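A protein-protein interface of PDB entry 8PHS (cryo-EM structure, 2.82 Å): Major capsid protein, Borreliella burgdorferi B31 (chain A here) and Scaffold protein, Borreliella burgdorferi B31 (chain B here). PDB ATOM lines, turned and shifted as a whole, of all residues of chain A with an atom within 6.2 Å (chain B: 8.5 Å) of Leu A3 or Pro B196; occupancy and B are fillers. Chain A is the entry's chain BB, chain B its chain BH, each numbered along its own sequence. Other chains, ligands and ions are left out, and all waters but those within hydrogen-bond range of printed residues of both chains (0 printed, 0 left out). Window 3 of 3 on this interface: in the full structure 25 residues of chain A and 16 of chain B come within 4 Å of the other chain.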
ATOM      1  N   LEU A   3      18.688  -6.378 -29.989  1.00  0.00           N
ATOM      2  CA  LEU A   3      17.955  -6.285 -28.732  1.00  0.00           C
ATOM      3  C   LEU A   3      16.637  -7.045 -28.809  1.00  0.00           C
ATOM      4  O   LEU A   3      16.270  -7.765 -27.881  1.00  0.00           O
ATOM      5  CB  LEU A   3      17.693  -4.823 -28.368  1.00  0.00           C
ATOM      6  CG  LEU A   3      16.591  -4.579 -27.335  1.00  0.00           C
ATOM      7  CD1 LEU A   3      17.088  -4.892 -25.934  1.00  0.00           C
ATOM      8  CD2 LEU A   3      16.074  -3.154 -27.420  1.00  0.00           C
ATOM      9  N   PHE A   4      15.930  -6.877 -29.927  1.00  0.00           N
ATOM     10  CA  PHE A   4      14.640  -7.535 -30.102  1.00  0.00           C
ATOM     11  C   PHE A   4      14.764  -9.051 -30.128  1.00  0.00           C
ATOM     12  O   PHE A   4      13.787  -9.748 -29.831  1.00  0.00           O
ATOM     13  CB  PHE A   4      13.975  -7.042 -31.386  1.00  0.00           C
ATOM     14  CG  PHE A   4      13.368  -5.673 -31.267  1.00  0.00           C
ATOM     15  CD1 PHE A   4      13.244  -5.063 -30.031  1.00  0.00           C
ATOM     16  CD2 PHE A   4      12.930  -4.996 -32.390  1.00  0.00           C
ATOM     17  CE1 PHE A   4      12.689  -3.804 -29.917  1.00  0.00           C
ATOM     18  CE2 PHE A   4      12.373  -3.736 -32.283  1.00  0.00           C
ATOM     19  CZ  PHE A   4      12.252  -3.141 -31.045  1.00  0.00           C
ATOM     20  N   ASP A   5      15.939  -9.578 -30.476  1.00  0.00           N
ATOM     21  CA  ASP A   5      16.136 -11.022 -30.464  1.00  0.00           C
ATOM     22  C   ASP A   5      16.185 -11.572 -29.045  1.00  0.00           C
ATOM     23  O   ASP A   5      15.791 -12.720 -28.813  1.00  0.00           O
ATOM     24  CB  ASP A   5      17.417 -11.380 -31.215  1.00  0.00           C
ATOM     25  CG  ASP A   5      17.359 -10.990 -32.678  1.00  0.00           C
ATOM     26  OD1 ASP A   5      16.289 -10.533 -33.129  1.00  0.00           O
ATOM     27  OD2 ASP A   5      18.384 -11.134 -33.375  1.00  0.00           O
ATOM     28  N   GLU A   6      16.660 -10.776 -28.089  1.00  0.00           N
ATOM     29  CA  GLU A   6      16.812 -11.208 -26.705  1.00  0.00           C
ATOM     30  C   GLU A   6      15.653 -10.769 -25.817  1.00  0.00           C
ATOM     31  O   GLU A   6      15.128 -11.574 -25.043  1.00  0.00           O
ATOM     32  CB  GLU A   6      18.132 -10.675 -26.135  1.00  0.00           C
ATOM     33  CG  GLU A   6      19.342 -10.976 -27.001  1.00  0.00           C
ATOM     34  CD  GLU A   6      20.547 -10.137 -26.628  1.00  0.00           C
ATOM     35  OE1 GLU A   6      20.417  -9.269 -25.740  1.00  0.00           O
ATOM     36  OE2 GLU A   6      21.624 -10.345 -27.225  1.00  0.00           O
ATOM     37  N   ASN A   7      15.246  -9.507 -25.910  1.00  0.00           N
ATOM     38  CA  ASN A   7      14.216  -8.945 -25.042  1.00  0.00           C
ATOM     39  C   ASN A   7      12.887  -8.949 -25.788  1.00  0.00           C
ATOM     40  O   ASN A   7      12.692  -8.170 -26.727  1.00  0.00           O
ATOM     41  CB  ASN A   7      14.598  -7.535 -24.598  1.00  0.00           C
ATOM     42  CG  ASN A   7      13.806  -7.067 -23.394  1.00  0.00           C
ATOM     43  OD1 ASN A   7      12.804  -7.672 -23.020  1.00  0.00           O
ATOM     44  ND2 ASN A   7      14.259  -5.984 -22.775  1.00  0.00           N
ATOM     45  N   TYR A   8      11.974  -9.826 -25.367  1.00  0.00           N
ATOM     46  CA  TYR A   8      10.656  -9.893 -25.988  1.00  0.00           C
ATOM     47  C   TYR A   8       9.766  -8.732 -25.569  1.00  0.00           C
ATOM     48  O   TYR A   8       8.916  -8.294 -26.353  1.00  0.00           O
ATOM     49  CB  TYR A   8       9.980 -11.222 -25.646  1.00  0.00           C
ATOM     50  CG  TYR A   8       8.468 -11.168 -25.673  1.00  0.00           C
ATOM     51  CD1 TYR A   8       7.771 -11.274 -26.870  1.00  0.00           C
ATOM     52  CD2 TYR A   8       7.736 -11.011 -24.503  1.00  0.00           C
ATOM     53  CE1 TYR A   8       6.391 -11.223 -26.900  1.00  0.00           C
ATOM     54  CE2 TYR A   8       6.356 -10.957 -24.524  1.00  0.00           C
ATOM     55  CZ  TYR A   8       5.689 -11.065 -25.723  1.00  0.00           C
ATOM     56  OH  TYR A   8       4.315 -11.014 -25.746  1.00  0.00           O
ATOM     57  N   ALA A  10      10.611  -5.602 -25.019  1.00  0.00           N
ATOM     58  CA  ALA A  10      10.919  -4.446 -25.853  1.00  0.00           C
ATOM     59  C   ALA A  10      10.264  -4.566 -27.223  1.00  0.00           C
ATOM     60  O   ALA A  10       9.711  -3.591 -27.743  1.00  0.00           O
ATOM     61  CB  ALA A  10      12.433  -4.288 -25.992  1.00  0.00           C
ATOM     62  N   GLU A 283      13.527  -1.269 -17.854  1.00  0.00           N
ATOM     63  CA  GLU A 283      14.206  -2.503 -18.234  1.00  0.00           C
ATOM     64  C   GLU A 283      13.989  -3.611 -17.212  1.00  0.00           C
ATOM     65  O   GLU A 283      14.012  -4.794 -17.571  1.00  0.00           O
ATOM     66  CB  GLU A 283      15.700  -2.245 -18.421  1.00  0.00           C
ATOM     67  CG  GLU A 283      16.400  -3.294 -19.264  1.00  0.00           C
ATOM     68  CD  GLU A 283      17.862  -2.975 -19.493  1.00  0.00           C
ATOM     69  OE1 GLU A 283      18.354  -1.985 -18.912  1.00  0.00           O
ATOM     70  OE2 GLU A 283      18.520  -3.714 -20.254  1.00  0.00           O
ATOM     71  N   ALA B 187      16.090   7.721 -35.661  1.00  0.00           N
ATOM     72  CA  ALA B 187      15.729   6.527 -34.907  1.00  0.00           C
ATOM     73  C   ALA B 187      14.303   6.628 -34.382  1.00  0.00           C
ATOM     74  O   ALA B 187      14.063   7.220 -33.331  1.00  0.00           O
ATOM     75  CB  ALA B 187      16.702   6.311 -33.760  1.00  0.00           C
ATOM     76  N   SER B 188      13.360   6.046 -35.118  1.00  0.00           N
ATOM     77  CA  SER B 188      11.951   6.077 -34.756  1.00  0.00           C
ATOM     78  C   SER B 188      11.341   4.696 -34.932  1.00  0.00           C
ATOM     79  O   SER B 188      11.682   3.972 -35.872  1.00  0.00           O
ATOM     80  CB  SER B 188      11.185   7.099 -35.606  1.00  0.00           C
ATOM     81  OG  SER B 188       9.805   7.098 -35.286  1.00  0.00           O
ATOM     82  N   LEU B 189      10.434   4.336 -34.021  1.00  0.00           N
ATOM     83  CA  LEU B 189       9.723   3.069 -34.137  1.00  0.00           C
ATOM     84  C   LEU B 189       8.792   3.041 -35.342  1.00  0.00           C
ATOM     85  O   LEU B 189       8.471   1.954 -35.835  1.00  0.00           O
ATOM     86  CB  LEU B 189       8.931   2.785 -32.862  1.00  0.00           C
ATOM     87  CG  LEU B 189       9.747   2.672 -31.574  1.00  0.00           C
ATOM     88  CD1 LEU B 189       8.855   2.283 -30.408  1.00  0.00           C
ATOM     89  CD2 LEU B 189      10.878   1.669 -31.743  1.00  0.00           C
ATOM     90  N   ASP B 191       9.599   4.117 -38.328  1.00  0.00           N
ATOM     91  CA  ASP B 191      10.477   3.601 -39.373  1.00  0.00           C
ATOM     92  C   ASP B 191      10.766   2.131 -39.096  1.00  0.00           C
ATOM     93  O   ASP B 191      11.508   1.801 -38.165  1.00  0.00           O
ATOM     94  CB  ASP B 191      11.766   4.414 -39.428  1.00  0.00           C
ATOM     95  CG  ASP B 191      12.687   3.972 -40.546  1.00  0.00           C
ATOM     96  OD1 ASP B 191      12.384   4.269 -41.720  1.00  0.00           O
ATOM     97  OD2 ASP B 191      13.716   3.329 -40.252  1.00  0.00           O
ATOM     98  N   SER B 192      10.181   1.244 -39.905  1.00  0.00           N
ATOM     99  CA  SER B 192      10.326  -0.190 -39.680  1.00  0.00           C
ATOM    100  C   SER B 192      11.760  -0.670 -39.868  1.00  0.00           C
ATOM    101  O   SER B 192      12.107  -1.748 -39.374  1.00  0.00           O
ATOM    102  CB  SER B 192       9.392  -0.964 -40.609  1.00  0.00           C
ATOM    103  OG  SER B 192       8.035  -0.676 -40.321  1.00  0.00           O
ATOM    104  N   ASN B 193      12.595   0.100 -40.567  1.00  0.00           N
ATOM    105  CA  ASN B 193      13.991  -0.275 -40.761  1.00  0.00           C
ATOM    106  C   ASN B 193      14.818  -0.149 -39.490  1.00  0.00           C
ATOM    107  O   ASN B 193      15.960  -0.621 -39.468  1.00  0.00           O
ATOM    108  CB  ASN B 193      14.612   0.580 -41.865  1.00  0.00           C
ATOM    109  CG  ASN B 193      13.804   0.552 -43.146  1.00  0.00           C
ATOM    110  OD1 ASN B 193      12.792  -0.142 -43.240  1.00  0.00           O
ATOM    111  ND2 ASN B 193      14.247   1.312 -44.141  1.00  0.00           N
ATOM    112  N   PHE B 194      14.282   0.474 -38.444  1.00  0.00           N
ATOM    113  CA  PHE B 194      15.033   0.682 -37.214  1.00  0.00           C
ATOM    114  C   PHE B 194      15.241  -0.645 -36.492  1.00  0.00           C
ATOM    115  O   PHE B 194      14.274  -1.342 -36.169  1.00  0.00           O
ATOM    116  CB  PHE B 194      14.301   1.671 -36.313  1.00  0.00           C
ATOM    117  CG  PHE B 194      14.866   1.760 -34.927  1.00  0.00           C
ATOM    118  CD1 PHE B 194      16.128   2.288 -34.714  1.00  0.00           C
ATOM    119  CD2 PHE B 194      14.141   1.310 -33.838  1.00  0.00           C
ATOM    120  CE1 PHE B 194      16.652   2.370 -33.440  1.00  0.00           C
ATOM    121  CE2 PHE B 194      14.660   1.387 -32.563  1.00  0.00           C
ATOM    122  CZ  PHE B 194      15.917   1.920 -32.363  1.00  0.00           C
ATOM    123  N   VAL B 195      16.496  -0.987 -36.238  1.00  0.00           N
ATOM    124  CA  VAL B 195      16.863  -2.173 -35.478  1.00  0.00           C
ATOM    125  C   VAL B 195      17.648  -1.725 -34.252  1.00  0.00           C
ATOM    126  O   VAL B 195      18.830  -1.393 -34.345  1.00  0.00           O
ATOM    127  CB  VAL B 195      17.679  -3.162 -36.332  1.00  0.00           C
ATOM    128  CG1 VAL B 195      18.216  -4.296 -35.468  1.00  0.00           C
ATOM    129  CG2 VAL B 195      16.827  -3.708 -37.467  1.00  0.00           C
ATOM    130  N   PRO B 196      17.013  -1.679 -33.084  1.00  0.00           N
ATOM    131  CA  PRO B 196      17.714  -1.211 -31.885  1.00  0.00           C
ATOM    132  C   PRO B 196      18.823  -2.163 -31.470  1.00  0.00           C
ATOM    133  O   PRO B 196      18.766  -3.371 -31.715  1.00  0.00           O
ATOM    134  CB  PRO B 196      16.609  -1.155 -30.823  1.00  0.00           C
ATOM    135  CG  PRO B 196      15.572  -2.100 -31.306  1.00  0.00           C
ATOM    136  CD  PRO B 196      15.617  -2.052 -32.804  1.00  0.00           C
ATOM    137  N   ILE B 197      19.847  -1.594 -30.838  1.00  0.00           N
ATOM    138  CA  ILE B 197      20.957  -2.383 -30.320  1.00  0.00           C
ATOM    139  C   ILE B 197      20.893  -2.542 -28.803  1.00  0.00           C
ATOM    140  O   ILE B 197      21.443  -3.519 -28.272  1.00  0.00           O
ATOM    141  CB  ILE B 197      22.307  -1.762 -30.736  1.00  0.00           C
ATOM    142  CG1 ILE B 197      22.251  -1.303 -32.193  1.00  0.00           C
ATOM    143  CG2 ILE B 197      23.439  -2.760 -30.555  1.00  0.00           C
ATOM    144  CD1 ILE B 197      23.492  -0.571 -32.651  1.00  0.00           C
ATOM    145  N   ASN B 198      20.229  -1.631 -28.096  1.00  0.00           N
ATOM    146  CA  ASN B 198      20.156  -1.703 -26.644  1.00  0.00           C
ATOM    147  C   ASN B 198      18.958  -0.901 -26.160  1.00  0.00           C
ATOM    148  O   ASN B 198      18.302  -0.186 -26.927  1.00  0.00           O
ATOM    149  CB  ASN B 198      21.453  -1.208 -25.999  1.00  0.00           C
ATOM    150  CG  ASN B 198      21.940   0.092 -26.600  1.00  0.00           C
ATOM    151  OD1 ASN B 198      21.375   1.155 -26.348  1.00  0.00           O
ATOM    152  ND2 ASN B 198      22.991   0.013 -27.406  1.00  0.00           N
ATOM    153  N   PHE B 199      18.681  -1.032 -24.860  1.00  0.00           N
ATOM    154  CA  PHE B 199      17.517  -0.379 -24.272  1.00  0.00           C
ATOM    155  C   PHE B 199      17.625   1.138 -24.341  1.00  0.00           C
ATOM    156  O   PHE B 199      16.602   1.828 -24.424  1.00  0.00           O
ATOM    157  CB  PHE B 199      17.339  -0.837 -22.825  1.00  0.00           C
ATOM    158  CG  PHE B 199      15.906  -0.902 -22.385  1.00  0.00           C
ATOM    159  CD1 PHE B 199      15.075  -1.908 -22.842  1.00  0.00           C
ATOM    160  CD2 PHE B 199      15.390   0.046 -21.520  1.00  0.00           C
ATOM    161  CE1 PHE B 199      13.756  -1.971 -22.441  1.00  0.00           C
ATOM    162  CE2 PHE B 199      14.072  -0.011 -21.116  1.00  0.00           C
ATOM    163  CZ  PHE B 199      13.254  -1.022 -21.577  1.00  0.00           C
ATOM    164  N   THR B 200      18.844   1.678 -24.309  1.00  0.00           N
ATOM    165  CA  THR B 200      19.017   3.121 -24.448  1.00  0.00           C
ATOM    166  C   THR B 200      18.516   3.602 -25.805  1.00  0.00           C
ATOM    167  O   THR B 200      17.736   4.561 -25.893  1.00  0.00           O
ATOM    168  CB  THR B 200      20.489   3.491 -24.255  1.00  0.00           C
ATOM    169  OG1 THR B 200      20.881   3.207 -22.906  1.00  0.00           O
ATOM    170  CG2 THR B 200      20.712   4.962 -24.548  1.00  0.00           C
ATOM    171  N   GLU B 201      18.949   2.937 -26.878  1.00  0.00           N
ATOM    172  CA  GLU B 201      18.471   3.290 -28.208  1.00  0.00           C
ATOM    173  C   GLU B 201      16.973   3.049 -28.331  1.00  0.00           C
ATOM    174  O   GLU B 201      16.271   3.800 -29.017  1.00  0.00           O
ATOM    175  CB  GLU B 201      19.230   2.499 -29.271  1.00  0.00           C
ATOM    176  CG  GLU B 201      20.731   2.719 -29.250  1.00  0.00           C
ATOM    177  CD  GLU B 201      21.431   2.041 -30.409  1.00  0.00           C
ATOM    178  OE1 GLU B 201      20.735   1.446 -31.258  1.00  0.00           O
ATOM    179  OE2 GLU B 201      22.677   2.103 -30.472  1.00  0.00           O
ATOM    180  N   PHE B 202      16.464   2.007 -27.671  1.00  0.00           N
ATOM    181  CA  PHE B 202      15.025   1.755 -27.695  1.00  0.00           C
ATOM    182  C   PHE B 202      14.249   2.914 -27.074  1.00  0.00           C
ATOM    183  O   PHE B 202      13.236   3.363 -27.624  1.00  0.00           O
ATOM    184  CB  PHE B 202      14.723   0.444 -26.970  1.00  0.00           C
ATOM    185  CG  PHE B 202      13.272   0.076 -26.959  1.00  0.00           C
ATOM    186  CD1 PHE B 202      12.565  -0.038 -28.142  1.00  0.00           C
ATOM    187  CD2 PHE B 202      12.616  -0.174 -25.766  1.00  0.00           C
ATOM    188  CE1 PHE B 202      11.230  -0.383 -28.135  1.00  0.00           C
ATOM    189  CE2 PHE B 202      11.282  -0.520 -25.754  1.00  0.00           C
ATOM    190  CZ  PHE B 202      10.587  -0.625 -26.940  1.00  0.00           C
ATOM    191  N   VAL B 203      14.722   3.421 -25.933  1.00  0.00           N
ATOM    192  CA  VAL B 203      14.050   4.534 -25.269  1.00  0.00           C
ATOM    193  C   VAL B 203      14.145   5.802 -26.112  1.00  0.00           C
ATOM    194  O   VAL B 203      13.178   6.573 -26.215  1.00  0.00           O
ATOM    195  CB  VAL B 203      14.634   4.739 -23.860  1.00  0.00           C
ATOM    196  CG1 VAL B 203      14.166   6.057 -23.270  1.00  0.00           C
ATOM    197  CG2 VAL B 203      14.240   3.583 -22.957  1.00  0.00           C
ATOM    198  N   GLN B 204      15.307   6.045 -26.723  1.00  0.00           N
ATOM    199  CA  GLN B 204      15.436   7.202 -27.607  1.00  0.00           C
ATOM    200  C   GLN B 204      14.468   7.107 -28.780  1.00  0.00           C
ATOM    201  O   GLN B 204      13.848   8.105 -29.169  1.00  0.00           O
ATOM    202  CB  GLN B 204      16.875   7.331 -28.107  1.00  0.00           C
ATOM    203  CG  GLN B 204      17.903   7.521 -27.007  1.00  0.00           C
ATOM    204  CD  GLN B 204      17.660   8.774 -26.192  1.00  0.00           C
ATOM    205  OE1 GLN B 204      17.700   9.886 -26.715  1.00  0.00           O
ATOM    206  NE2 GLN B 204      17.405   8.598 -24.901  1.00  0.00           N
ATOM    207  N   ALA B 205      14.322   5.910 -29.353  1.00  0.00           N
ATOM    208  CA  ALA B 205      13.372   5.716 -30.442  1.00  0.00           C
ATOM    209  C   ALA B 205      11.943   5.957 -29.977  1.00  0.00           C
ATOM    210  O   ALA B 205      11.130   6.519 -30.719  1.00  0.00           O
ATOM    211  CB  ALA B 205      13.517   4.312 -31.022  1.00  0.00           C
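The backbone carbonyl oxygen of Pro B196 lies within hydrogen-bond range of the backbone NH of Leu A3.
The side-chain amide oxygen (OD1) of Asn B198 lies close to the backbone NH (N) of Thr B200, 3.3 Å away.
The backbone NH (N) of Ile B197 sits at hydrogen-bond distance from the side-chain carboxylate (OE1) of Glu B201, at 3.2 Å.
OD1 of Asn B198 sits at hydrogen-bond distance from N of Glu B201, 3.1 Å away.
Ile B197 touches Leu A3.
Leu A3 touches Asn B198.
CB of Phe B202 touches CD2 of Leu A3, 3.9 Å away.
Phe A4 touches Pro B196 (CZ to CG, 3.5 Å).
Phe B202 touches Ala A10.
Phe B199 touches Glu A283.
Of the printed residues of chain B, Leu A3 touches Pro B196 (3.5 Å), Ile B197 (3.95 Å), Asn B198 (3.7 Å) and Phe B202 (3.9 Å).
Printed residues of chain B within 4 Å of Phe A4: Pro B196.
Printed residues of chain B within 4 Å of Glu A283: Phe B199 (3.5 Å).
Printed residues of chain A within 4 Å of Ile B197: Leu A3 (3.95 Å).
Of the printed residues of chain A, Asn B198 touches Leu A3 (3.7 Å).
Of the printed residues of chain A, Phe B199 touches Glu A283.
Of the printed residues of chain A, Phe B202 touches Leu A3 and Ala A10.
The nearest printed residue of chain B that does not touch Ala A10 is Phe B199 (4.4 Å).
Of the 18 printed residues of chain B, 5 touch a printed residue of chain A.
Printed residues of chain B that touch a printed residue of chain A: Pro B196, Ile B197, Asn B198, Phe B199 and Phe B202.
Hydrophobic or aromatic side chains of chain B within 4 Å of the printed part of chain A: Pro B196, Phe B199 and Phe B202.
Among the printed residues, no Asp or Glu carboxylate lies within 4 Å of a Lys or Arg side-chain nitrogen of the other chain.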
